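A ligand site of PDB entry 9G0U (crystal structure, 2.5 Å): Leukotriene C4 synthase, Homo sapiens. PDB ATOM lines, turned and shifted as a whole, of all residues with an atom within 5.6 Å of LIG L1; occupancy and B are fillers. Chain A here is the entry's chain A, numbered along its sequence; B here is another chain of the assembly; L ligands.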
ATOM      1  N   ASN A  62     -18.328  17.919  17.559  1.00  0.00           N
ATOM      2  CA  ASN A  62     -17.343  18.865  17.011  1.00  0.00           C
ATOM      3  C   ASN A  62     -16.321  19.306  18.026  1.00  0.00           C
ATOM      4  O   ASN A  62     -15.133  19.243  17.745  1.00  0.00           O
ATOM      5  CB  ASN A  62     -18.037  20.048  16.356  1.00  0.00           C
ATOM      6  CG  ASN A  62     -18.826  19.656  15.148  1.00  0.00           C
ATOM      7  OD1 ASN A  62     -18.446  18.790  14.391  1.00  0.00           O
ATOM      8  ND2 ASN A  62     -19.957  20.293  14.943  1.00  0.00           N
ATOM      9  N   TYR A  66     -12.054  18.339  18.181  1.00  0.00           N
ATOM     10  CA  TYR A  66     -11.062  19.388  18.313  1.00  0.00           C
ATOM     11  C   TYR A  66     -10.382  19.475  19.662  1.00  0.00           C
ATOM     12  O   TYR A  66      -9.288  20.036  19.731  1.00  0.00           O
ATOM     13  CB  TYR A  66     -11.703  20.728  17.941  1.00  0.00           C
ATOM     14  CG  TYR A  66     -11.807  20.862  16.436  1.00  0.00           C
ATOM     15  CD1 TYR A  66     -10.722  21.300  15.686  1.00  0.00           C
ATOM     16  CD2 TYR A  66     -12.939  20.428  15.759  1.00  0.00           C
ATOM     17  CE1 TYR A  66     -10.775  21.357  14.302  1.00  0.00           C
ATOM     18  CE2 TYR A  66     -13.001  20.457  14.367  1.00  0.00           C
ATOM     19  CZ  TYR A  66     -11.920  20.932  13.644  1.00  0.00           C
ATOM     20  OH  TYR A  66     -11.935  20.968  12.286  1.00  0.00           O
ATOM     21  N   LEU A  69      -6.704  18.353  19.498  1.00  0.00           N
ATOM     22  CA  LEU A  69      -5.971  19.341  18.661  1.00  0.00           C
ATOM     23  C   LEU A  69      -5.623  20.554  19.506  1.00  0.00           C
ATOM     24  O   LEU A  69      -4.487  21.034  19.474  1.00  0.00           O
ATOM     25  CB  LEU A  69      -6.875  19.774  17.467  1.00  0.00           C
ATOM     26  CG  LEU A  69      -6.656  19.034  16.126  1.00  0.00           C
ATOM     27  CD1 LEU A  69      -6.626  17.570  16.277  1.00  0.00           C
ATOM     28  CD2 LEU A  69      -7.715  19.440  15.112  1.00  0.00           C
ATOM     29  N   TYR A  93     -10.039  30.274  23.415  1.00  0.00           N
ATOM     30  CA  TYR A  93     -10.525  29.135  22.652  1.00  0.00           C
ATOM     31  C   TYR A  93     -11.634  28.419  23.408  1.00  0.00           C
ATOM     32  O   TYR A  93     -12.700  28.117  22.832  1.00  0.00           O
ATOM     33  CB  TYR A  93      -9.357  28.161  22.282  1.00  0.00           C
ATOM     34  CG  TYR A  93      -9.876  26.905  21.615  1.00  0.00           C
ATOM     35  CD1 TYR A  93     -10.223  26.907  20.261  1.00  0.00           C
ATOM     36  CD2 TYR A  93     -10.184  25.773  22.359  1.00  0.00           C
ATOM     37  CE1 TYR A  93     -10.782  25.766  19.653  1.00  0.00           C
ATOM     38  CE2 TYR A  93     -10.762  24.652  21.775  1.00  0.00           C
ATOM     39  CZ  TYR A  93     -11.058  24.650  20.416  1.00  0.00           C
ATOM     40  OH  TYR A  93     -11.562  23.518  19.863  1.00  0.00           O
ATOM     41  N   ARG A  97     -15.731  28.279  22.537  1.00  0.00           N
ATOM     42  CA  ARG A  97     -16.369  26.998  22.319  1.00  0.00           C
ATOM     43  C   ARG A  97     -17.627  26.862  23.132  1.00  0.00           C
ATOM     44  O   ARG A  97     -18.565  26.241  22.702  1.00  0.00           O
ATOM     45  CB  ARG A  97     -15.399  25.872  22.605  1.00  0.00           C
ATOM     46  CG  ARG A  97     -14.437  25.646  21.471  1.00  0.00           C
ATOM     47  CD  ARG A  97     -14.984  24.613  20.545  1.00  0.00           C
ATOM     48  NE  ARG A  97     -14.758  24.950  19.163  1.00  0.00           N
ATOM     49  CZ  ARG A  97     -15.067  24.147  18.162  1.00  0.00           C
ATOM     50  NH1 ARG A  97     -14.839  24.509  16.946  1.00  0.00           N
ATOM     51  NH2 ARG A  97     -15.608  22.990  18.392  1.00  0.00           N
ATOM     52  N   TYR A 100     -20.057  28.821  21.138  1.00  0.00           N
ATOM     53  CA  TYR A 100     -20.330  28.024  19.939  1.00  0.00           C
ATOM     54  C   TYR A 100     -21.440  27.035  20.269  1.00  0.00           C
ATOM     55  O   TYR A 100     -22.442  26.918  19.528  1.00  0.00           O
ATOM     56  CB  TYR A 100     -19.026  27.277  19.511  1.00  0.00           C
ATOM     57  CG  TYR A 100     -19.246  26.104  18.578  1.00  0.00           C
ATOM     58  CD1 TYR A 100     -19.558  26.312  17.232  1.00  0.00           C
ATOM     59  CD2 TYR A 100     -19.177  24.793  19.038  1.00  0.00           C
ATOM     60  CE1 TYR A 100     -19.785  25.241  16.366  1.00  0.00           C
ATOM     61  CE2 TYR A 100     -19.392  23.717  18.178  1.00  0.00           C
ATOM     62  CZ  TYR A 100     -19.683  23.946  16.845  1.00  0.00           C
ATOM     63  OH  TYR A 100     -19.892  22.901  15.984  1.00  0.00           O
ATOM     64  N   TYR A 104     -25.101  27.213  18.697  1.00  0.00           N
ATOM     65  CA  TYR A 104     -25.518  26.038  17.910  1.00  0.00           C
ATOM     66  C   TYR A 104     -26.786  25.394  18.462  1.00  0.00           C
ATOM     67  O   TYR A 104     -27.630  24.989  17.667  1.00  0.00           O
ATOM     68  CB  TYR A 104     -24.382  25.006  17.862  1.00  0.00           C
ATOM     69  CG  TYR A 104     -24.314  24.129  16.631  1.00  0.00           C
ATOM     70  CD1 TYR A 104     -25.397  24.040  15.745  1.00  0.00           C
ATOM     71  CD2 TYR A 104     -23.216  23.300  16.397  1.00  0.00           C
ATOM     72  CE1 TYR A 104     -25.339  23.218  14.629  1.00  0.00           C
ATOM     73  CE2 TYR A 104     -23.161  22.468  15.278  1.00  0.00           C
ATOM     74  CZ  TYR A 104     -24.222  22.440  14.388  1.00  0.00           C
ATOM     75  OH  TYR A 104     -24.155  21.645  13.281  1.00  0.00           O
ATOM     76  N   ARG A 111     -24.161  29.749  15.693  1.00  0.00           N
ATOM     77  CA  ARG A 111     -22.923  29.053  16.044  1.00  0.00           C
ATOM     78  C   ARG A 111     -21.709  29.668  15.362  1.00  0.00           C
ATOM     79  O   ARG A 111     -20.588  29.505  15.854  1.00  0.00           O
ATOM     80  CB  ARG A 111     -23.023  27.554  15.670  1.00  0.00           C
ATOM     81  CG  ARG A 111     -22.350  27.134  14.340  1.00  0.00           C
ATOM     82  CD  ARG A 111     -22.829  25.781  13.833  1.00  0.00           C
ATOM     83  NE  ARG A 111     -22.047  25.302  12.682  1.00  0.00           N
ATOM     84  CZ  ARG A 111     -22.300  25.598  11.411  1.00  0.00           C
ATOM     85  NH1 ARG A 111     -21.538  25.100  10.447  1.00  0.00           N
ATOM     86  NH2 ARG A 111     -23.296  26.403  11.090  1.00  0.00           N
ATOM     87  N   LEU A 115     -17.786  30.243  16.395  1.00  0.00           N
ATOM     88  CA  LEU A 115     -17.006  29.216  15.691  1.00  0.00           C
ATOM     89  C   LEU A 115     -15.789  29.870  15.024  1.00  0.00           C
ATOM     90  O   LEU A 115     -14.698  29.317  15.107  1.00  0.00           O
ATOM     91  CB  LEU A 115     -17.881  28.491  14.618  1.00  0.00           C
ATOM     92  CG  LEU A 115     -17.187  27.493  13.670  1.00  0.00           C
ATOM     93  CD1 LEU A 115     -16.414  26.437  14.434  1.00  0.00           C
ATOM     94  CD2 LEU A 115     -18.183  26.851  12.778  1.00  0.00           C
ATOM     95  N   SER A 118     -13.290  30.902  17.744  1.00  0.00           N
ATOM     96  CA  SER A 118     -12.563  29.716  18.199  1.00  0.00           C
ATOM     97  C   SER A 118     -11.530  29.237  17.165  1.00  0.00           C
ATOM     98  O   SER A 118     -10.447  28.751  17.535  1.00  0.00           O
ATOM     99  CB  SER A 118     -13.530  28.617  18.622  1.00  0.00           C
ATOM    100  OG  SER A 118     -13.938  27.820  17.529  1.00  0.00           O
ATOM    101  N   ALA A 119     -11.859  29.381  15.865  1.00  0.00           N
ATOM    102  CA  ALA A 119     -10.991  29.036  14.721  1.00  0.00           C
ATOM    103  C   ALA A 119      -9.805  30.007  14.719  1.00  0.00           C
ATOM    104  O   ALA A 119      -8.653  29.581  14.546  1.00  0.00           O
ATOM    105  CB  ALA A 119     -11.780  29.166  13.425  1.00  0.00           C
ATOM    106  N   ARG A 120     -10.080  31.307  14.963  1.00  0.00           N
ATOM    107  CA  ARG A 120      -9.061  32.350  15.085  1.00  0.00           C
ATOM    108  C   ARG A 120      -8.112  32.050  16.264  1.00  0.00           C
ATOM    109  O   ARG A 120      -6.908  32.136  16.084  1.00  0.00           O
ATOM    110  CB  ARG A 120      -9.726  33.737  15.254  1.00  0.00           C
ATOM    111  CG  ARG A 120      -9.946  34.463  13.948  1.00  0.00           C
ATOM    112  CD  ARG A 120     -10.547  35.840  14.151  1.00  0.00           C
ATOM    113  NE  ARG A 120     -11.919  35.871  13.645  1.00  0.00           N
ATOM    114  CZ  ARG A 120     -13.000  36.001  14.404  1.00  0.00           C
ATOM    115  NH1 ARG A 120     -14.202  35.990  13.853  1.00  0.00           N
ATOM    116  NH2 ARG A 120     -12.887  36.199  15.717  1.00  0.00           N
ATOM    117  N   LEU A 122      -7.570  29.031  17.811  1.00  0.00           N
ATOM    118  CA  LEU A 122      -6.823  27.794  17.567  1.00  0.00           C
ATOM    119  C   LEU A 122      -5.668  27.991  16.563  1.00  0.00           C
ATOM    120  O   LEU A 122      -4.606  27.385  16.744  1.00  0.00           O
ATOM    121  CB  LEU A 122      -7.750  26.638  17.149  1.00  0.00           C
ATOM    122  CG  LEU A 122      -7.185  25.198  17.289  1.00  0.00           C
ATOM    123  CD1 LEU A 122      -6.709  24.912  18.712  1.00  0.00           C
ATOM    124  CD2 LEU A 122      -8.189  24.155  16.805  1.00  0.00           C
ATOM    125  N   TRP A 123      -5.879  28.821  15.510  1.00  0.00           N
ATOM    126  CA  TRP A 123      -4.857  29.150  14.508  1.00  0.00           C
ATOM    127  C   TRP A 123      -3.758  29.975  15.166  1.00  0.00           C
ATOM    128  O   TRP A 123      -2.576  29.781  14.855  1.00  0.00           O
ATOM    129  CB  TRP A 123      -5.454  29.926  13.299  1.00  0.00           C
ATOM    130  CG  TRP A 123      -6.015  29.042  12.226  1.00  0.00           C
ATOM    131  CD1 TRP A 123      -7.269  29.093  11.704  1.00  0.00           C
ATOM    132  CD2 TRP A 123      -5.342  27.964  11.554  1.00  0.00           C
ATOM    133  NE1 TRP A 123      -7.427  28.120  10.735  1.00  0.00           N
ATOM    134  CE2 TRP A 123      -6.264  27.402  10.640  1.00  0.00           C
ATOM    135  CE3 TRP A 123      -4.048  27.414  11.624  1.00  0.00           C
ATOM    136  CZ2 TRP A 123      -5.938  26.314   9.807  1.00  0.00           C
ATOM    137  CZ3 TRP A 123      -3.732  26.332  10.819  1.00  0.00           C
ATOM    138  CH2 TRP A 123      -4.664  25.801   9.920  1.00  0.00           C
ATOM    139  N   VAL A 126      -1.698  27.480  16.946  1.00  0.00           N
ATOM    140  CA  VAL A 126      -0.888  26.783  15.932  1.00  0.00           C
ATOM    141  C   VAL A 126       0.329  27.698  15.551  1.00  0.00           C
ATOM    142  O   VAL A 126       1.468  27.222  15.517  1.00  0.00           O
ATOM    143  CB  VAL A 126      -1.738  26.352  14.703  1.00  0.00           C
ATOM    144  CG1 VAL A 126      -0.853  25.893  13.553  1.00  0.00           C
ATOM    145  CG2 VAL A 126      -2.727  25.244  15.073  1.00  0.00           C
ATOM    146  N   VAL B  23      -1.550  18.023  13.478  1.00  0.00           N
ATOM    147  CA  VAL B  23      -2.621  18.988  13.704  1.00  0.00           C
ATOM    148  C   VAL B  23      -2.960  19.647  12.350  1.00  0.00           C
ATOM    149  O   VAL B  23      -4.136  19.775  11.993  1.00  0.00           O
ATOM    150  CB  VAL B  23      -2.200  20.015  14.820  1.00  0.00           C
ATOM    151  CG1 VAL B  23      -3.169  21.199  14.906  1.00  0.00           C
ATOM    152  CG2 VAL B  23      -2.037  19.321  16.190  1.00  0.00           C
ATOM    153  N   LEU B  24      -1.934  20.029  11.593  1.00  0.00           N
ATOM    154  CA  LEU B  24      -2.042  20.647  10.266  1.00  0.00           C
ATOM    155  C   LEU B  24      -2.699  19.710   9.255  1.00  0.00           C
ATOM    156  O   LEU B  24      -3.510  20.186   8.455  1.00  0.00           O
ATOM    157  CB  LEU B  24      -0.660  21.146   9.778  1.00  0.00           C
ATOM    158  CG  LEU B  24      -0.114  22.425  10.447  1.00  0.00           C
ATOM    159  CD1 LEU B  24       1.259  22.754   9.915  1.00  0.00           C
ATOM    160  CD2 LEU B  24      -1.048  23.647  10.202  1.00  0.00           C
ATOM    161  N   ALA B  27      -6.349  19.728   9.998  1.00  0.00           N
ATOM    162  CA  ALA B  27      -6.941  20.956   9.442  1.00  0.00           C
ATOM    163  C   ALA B  27      -7.200  20.783   7.958  1.00  0.00           C
ATOM    164  O   ALA B  27      -8.249  21.203   7.484  1.00  0.00           O
ATOM    165  CB  ALA B  27      -6.055  22.167   9.694  1.00  0.00           C
ATOM    166  N   TYR B  28      -6.297  20.077   7.226  1.00  0.00           N
ATOM    167  CA  TYR B  28      -6.439  19.793   5.797  1.00  0.00           C
ATOM    168  C   TYR B  28      -7.651  18.911   5.507  1.00  0.00           C
ATOM    169  O   TYR B  28      -8.399  19.199   4.577  1.00  0.00           O
ATOM    170  CB  TYR B  28      -5.150  19.195   5.188  1.00  0.00           C
ATOM    171  CG  TYR B  28      -5.322  18.724   3.757  1.00  0.00           C
ATOM    172  CD1 TYR B  28      -5.460  19.638   2.706  1.00  0.00           C
ATOM    173  CD2 TYR B  28      -5.402  17.364   3.446  1.00  0.00           C
ATOM    174  CE1 TYR B  28      -5.666  19.208   1.392  1.00  0.00           C
ATOM    175  CE2 TYR B  28      -5.615  16.931   2.143  1.00  0.00           C
ATOM    176  CZ  TYR B  28      -5.738  17.853   1.125  1.00  0.00           C
ATOM    177  OH  TYR B  28      -5.916  17.417  -0.167  1.00  0.00           O
ATOM    178  N   SER B  30     -10.281  18.492   7.408  1.00  0.00           N
ATOM    179  CA  SER B  30     -11.403  19.359   7.788  1.00  0.00           C
ATOM    180  C   SER B  30     -11.806  20.312   6.617  1.00  0.00           C
ATOM    181  O   SER B  30     -13.001  20.480   6.361  1.00  0.00           O
ATOM    182  CB  SER B  30     -11.026  20.138   9.039  1.00  0.00           C
ATOM    183  OG  SER B  30     -11.868  21.268   9.233  1.00  0.00           O
ATOM    184  N   LEU B  31     -10.809  20.888   5.904  1.00  0.00           N
ATOM    185  CA  LEU B  31     -10.982  21.770   4.749  1.00  0.00           C
ATOM    186  C   LEU B  31     -11.658  21.006   3.590  1.00  0.00           C
ATOM    187  O   LEU B  31     -12.534  21.549   2.926  1.00  0.00           O
ATOM    188  CB  LEU B  31      -9.602  22.305   4.321  1.00  0.00           C
ATOM    189  CG  LEU B  31      -9.495  23.163   3.053  1.00  0.00           C
ATOM    190  CD1 LEU B  31      -9.890  24.602   3.334  1.00  0.00           C
ATOM    191  CD2 LEU B  31      -8.092  23.133   2.544  1.00  0.00           C
ATOM    192  N   ILE B  34     -15.381  20.455   4.401  1.00  0.00           N
ATOM    193  CA  ILE B  34     -16.052  21.749   4.176  1.00  0.00           C
ATOM    194  C   ILE B  34     -16.364  21.916   2.678  1.00  0.00           C
ATOM    195  O   ILE B  34     -17.460  22.370   2.321  1.00  0.00           O
ATOM    196  CB  ILE B  34     -15.213  22.941   4.746  1.00  0.00           C
ATOM    197  CG1 ILE B  34     -15.229  22.971   6.274  1.00  0.00           C
ATOM    198  CG2 ILE B  34     -15.633  24.307   4.164  1.00  0.00           C
ATOM    199  CD1 ILE B  34     -14.022  23.680   6.909  1.00  0.00           C
ATOM    200  N   PRO B  44     -25.117  21.673   7.774  1.00  0.00           N
ATOM    201  CA  PRO B  44     -25.093  21.344   9.176  1.00  0.00           C
ATOM    202  C   PRO B  44     -26.482  21.579   9.754  1.00  0.00           C
ATOM    203  O   PRO B  44     -27.000  22.640   9.546  1.00  0.00           O
ATOM    204  CB  PRO B  44     -24.105  22.388   9.676  1.00  0.00           C
ATOM    205  CG  PRO B  44     -23.150  22.551   8.537  1.00  0.00           C
ATOM    206  CD  PRO B  44     -24.077  22.605   7.350  1.00  0.00           C
HETATM  207  C1  LIG L   1      -9.176  25.872  12.592  1.00  0.00           C
HETATM  208  C2  LIG L   1      -8.079  26.251  13.380  1.00  0.00           C
HETATM  209  C3  LIG L   1      -7.051  25.312  13.569  1.00  0.00           C
HETATM  210  C4  LIG L   1     -10.144  23.769   9.883  1.00  0.00           C
HETATM  211  C5  LIG L   1     -10.068  24.908   8.839  1.00  0.00           C
HETATM  212  C6  LIG L   1      -9.846  24.313   7.422  1.00  0.00           C
HETATM  213  C7  LIG L   1     -11.307  25.851   8.893  1.00  0.00           C
HETATM  214  C8  LIG L   1     -13.991  23.747  13.129  1.00  0.00           C
HETATM  215  C9  LIG L   1     -12.873  24.253  13.840  1.00  0.00           C
HETATM  216  C10 LIG L   1     -11.586  24.156  11.849  1.00  0.00           C
HETATM  217  C11 LIG L   1     -12.706  23.683  11.140  1.00  0.00           C
HETATM  218  C12 LIG L   1     -11.852  25.361  15.778  1.00  0.00           C
HETATM  219  C13 LIG L   1     -17.780  22.695  13.439  1.00  0.00           C
HETATM  220  C14 LIG L   1     -17.028  21.548  12.727  1.00  0.00           C
HETATM  221  C15 LIG L   1     -16.432  22.968  12.757  1.00  0.00           C
HETATM  222  C16 LIG L   1     -18.964  23.369  12.784  1.00  0.00           C
HETATM  223  C17 LIG L   1     -15.321  23.323  13.710  1.00  0.00           C
HETATM  224  C18 LIG L   1      -7.172  24.033  13.046  1.00  0.00           C
HETATM  225  C19 LIG L   1      -8.264  23.647  12.275  1.00  0.00           C
HETATM  226  C20 LIG L   1      -9.271  24.587  12.025  1.00  0.00           C
HETATM  227  F1  LIG L   1      -5.932  25.597  14.179  1.00  0.00           F
HETATM  228 CL1  LIG L   1      -5.835  22.970  13.374  1.00  0.00          CL
HETATM  229  F2  LIG L   1     -10.140  26.730  12.385  1.00  0.00           F
HETATM  230  N1  LIG L   1     -10.360  24.240  11.269  1.00  0.00           N
HETATM  231  F3  LIG L   1      -9.014  25.696   9.137  1.00  0.00           F
HETATM  232  N2  LIG L   1     -11.723  24.445  13.171  1.00  0.00           N
HETATM  233  N3  LIG L   1     -13.851  23.467  11.809  1.00  0.00           N
HETATM  234  O1  LIG L   1     -12.891  24.553  15.211  1.00  0.00           O
HETATM  235  O2  LIG L   1     -15.479  23.146  14.893  1.00  0.00           O
HETATM  236  O3  LIG L   1     -19.920  23.728  13.455  1.00  0.00           O
HETATM  237  O4  LIG L   1     -18.893  23.585  11.464  1.00  0.00           O
HETATM  238  C1  LG2 L   2     -26.914  26.240   4.720  1.00  0.00           C
HETATM  239  O1  LG2 L   2     -26.635  27.536   4.499  1.00  0.00           O
HETATM  240  O2  LG2 L   2     -28.053  25.791   4.553  1.00  0.00           O
HETATM  241  C2  LG2 L   2     -25.723  25.393   5.146  1.00  0.00           C
HETATM  242  C3  LG2 L   2     -24.329  26.027   4.844  1.00  0.00           C
HETATM  243  C4  LG2 L   2     -23.148  25.488   5.735  1.00  0.00           C
HETATM  244  C5  LG2 L   2     -22.830  26.379   6.971  1.00  0.00           C
HETATM  245  C6  LG2 L   2     -21.342  26.805   6.949  1.00  0.00           C
HETATM  246  C7  LG2 L   2     -20.291  25.822   7.572  1.00  0.00           C
HETATM  247  C8  LG2 L   2     -19.032  26.621   8.005  1.00  0.00           C
HETATM  248  C9  LG2 L   2     -18.133  25.853   8.940  1.00  0.00           C
HETATM  249  C10 LG2 L   2     -16.869  26.099   9.379  1.00  0.00           C
HETATM  250  C11 LG2 L   2     -15.901  27.235   9.083  1.00  0.00           C
HETATM  251  C12 LG2 L   2     -14.681  27.141  10.055  1.00  0.00           C
HETATM  252  C13 LG2 L   2     -14.056  28.536  10.379  1.00  0.00           C
HETATM  253  C14 LG2 L   2     -12.995  29.017   9.340  1.00  0.00           C
HETATM  254  C15 LG2 L   2     -12.114  30.203   9.851  1.00  0.00           C
HETATM  255  C16 LG2 L   2     -10.676  30.191   9.249  1.00  0.00           C
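O2 of LIG L1 is in hydrogen-bond range of NH1 of Arg 97 (2.5 Å). An oxygen (O3) of LIG L1 is in hydrogen-bond range of the side-chain hydroxyl of Tyr 100 (2.7 Å). NE of Arg 111 lies within salt-bridge range of O3 of LIG L1, 2.8 Å away. OH of Tyr 66 lies close to N3 of LIG L1, at 3.2 Å.
The guanidinium group (NE) of Arg 97 is in hydrogen-bond range of the side-chain hydroxyl (OG) of Ser 118, at 3.4 Å. The side-chain hydroxyl (OH) of Tyr 100 is in hydrogen-bond range of the side-chain amide nitrogen (ND2) of Asn 62. OH of Tyr 66 is in hydrogen-bond range of OG of Ser 30 of chain B (3.1 Å). OG of Ser 118 sits at hydrogen-bond distance from O of Leu 115, at 2.9 Å.
A fluorine (F1) of LIG L1 lies close to the backbone carbonyl oxygen of Leu 122, at 3.4 Å. NE1 of Trp 123 sits close to F3 of LIG L1 (3.3 Å). Asn 62 touches LIG L1. CE2 of Tyr 104 touches O3 of LIG L1, at 3.9 Å. Leu 115 touches LIG L1 (CD1 to C17, 3.4 Å). Ser 118 touches LIG L1. Ala 119 touches LIG L1 (CB to F2, 3.1 Å). CG2 of Val 126 touches F1 of LIG L1 (3.3 Å). Val 23 of chain B touches LIG L1. Ala 27 of chain B touches LIG L1 (O to C6, 3.5 Å). Ser 30 of chain B touches LIG L1. CB of Leu 31 of chain B touches C6 of LIG L1, 3.7 Å away. Hydrophobic or aromatic side chains within 4 Å of LIG L1: Tyr 66, Tyr 100, Tyr 104, Leu 115, Ala 119, Leu 122, Trp 123, Val 126, Val 23 of chain B, Ala 27 of chain B and Leu 31 of chain B. Of the 23 residues printed, 16 come within 4 Å of LIG L1. The nearest printed residue that does not touch LIG L1 is Ile 34 of chain B (4.003 Å).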
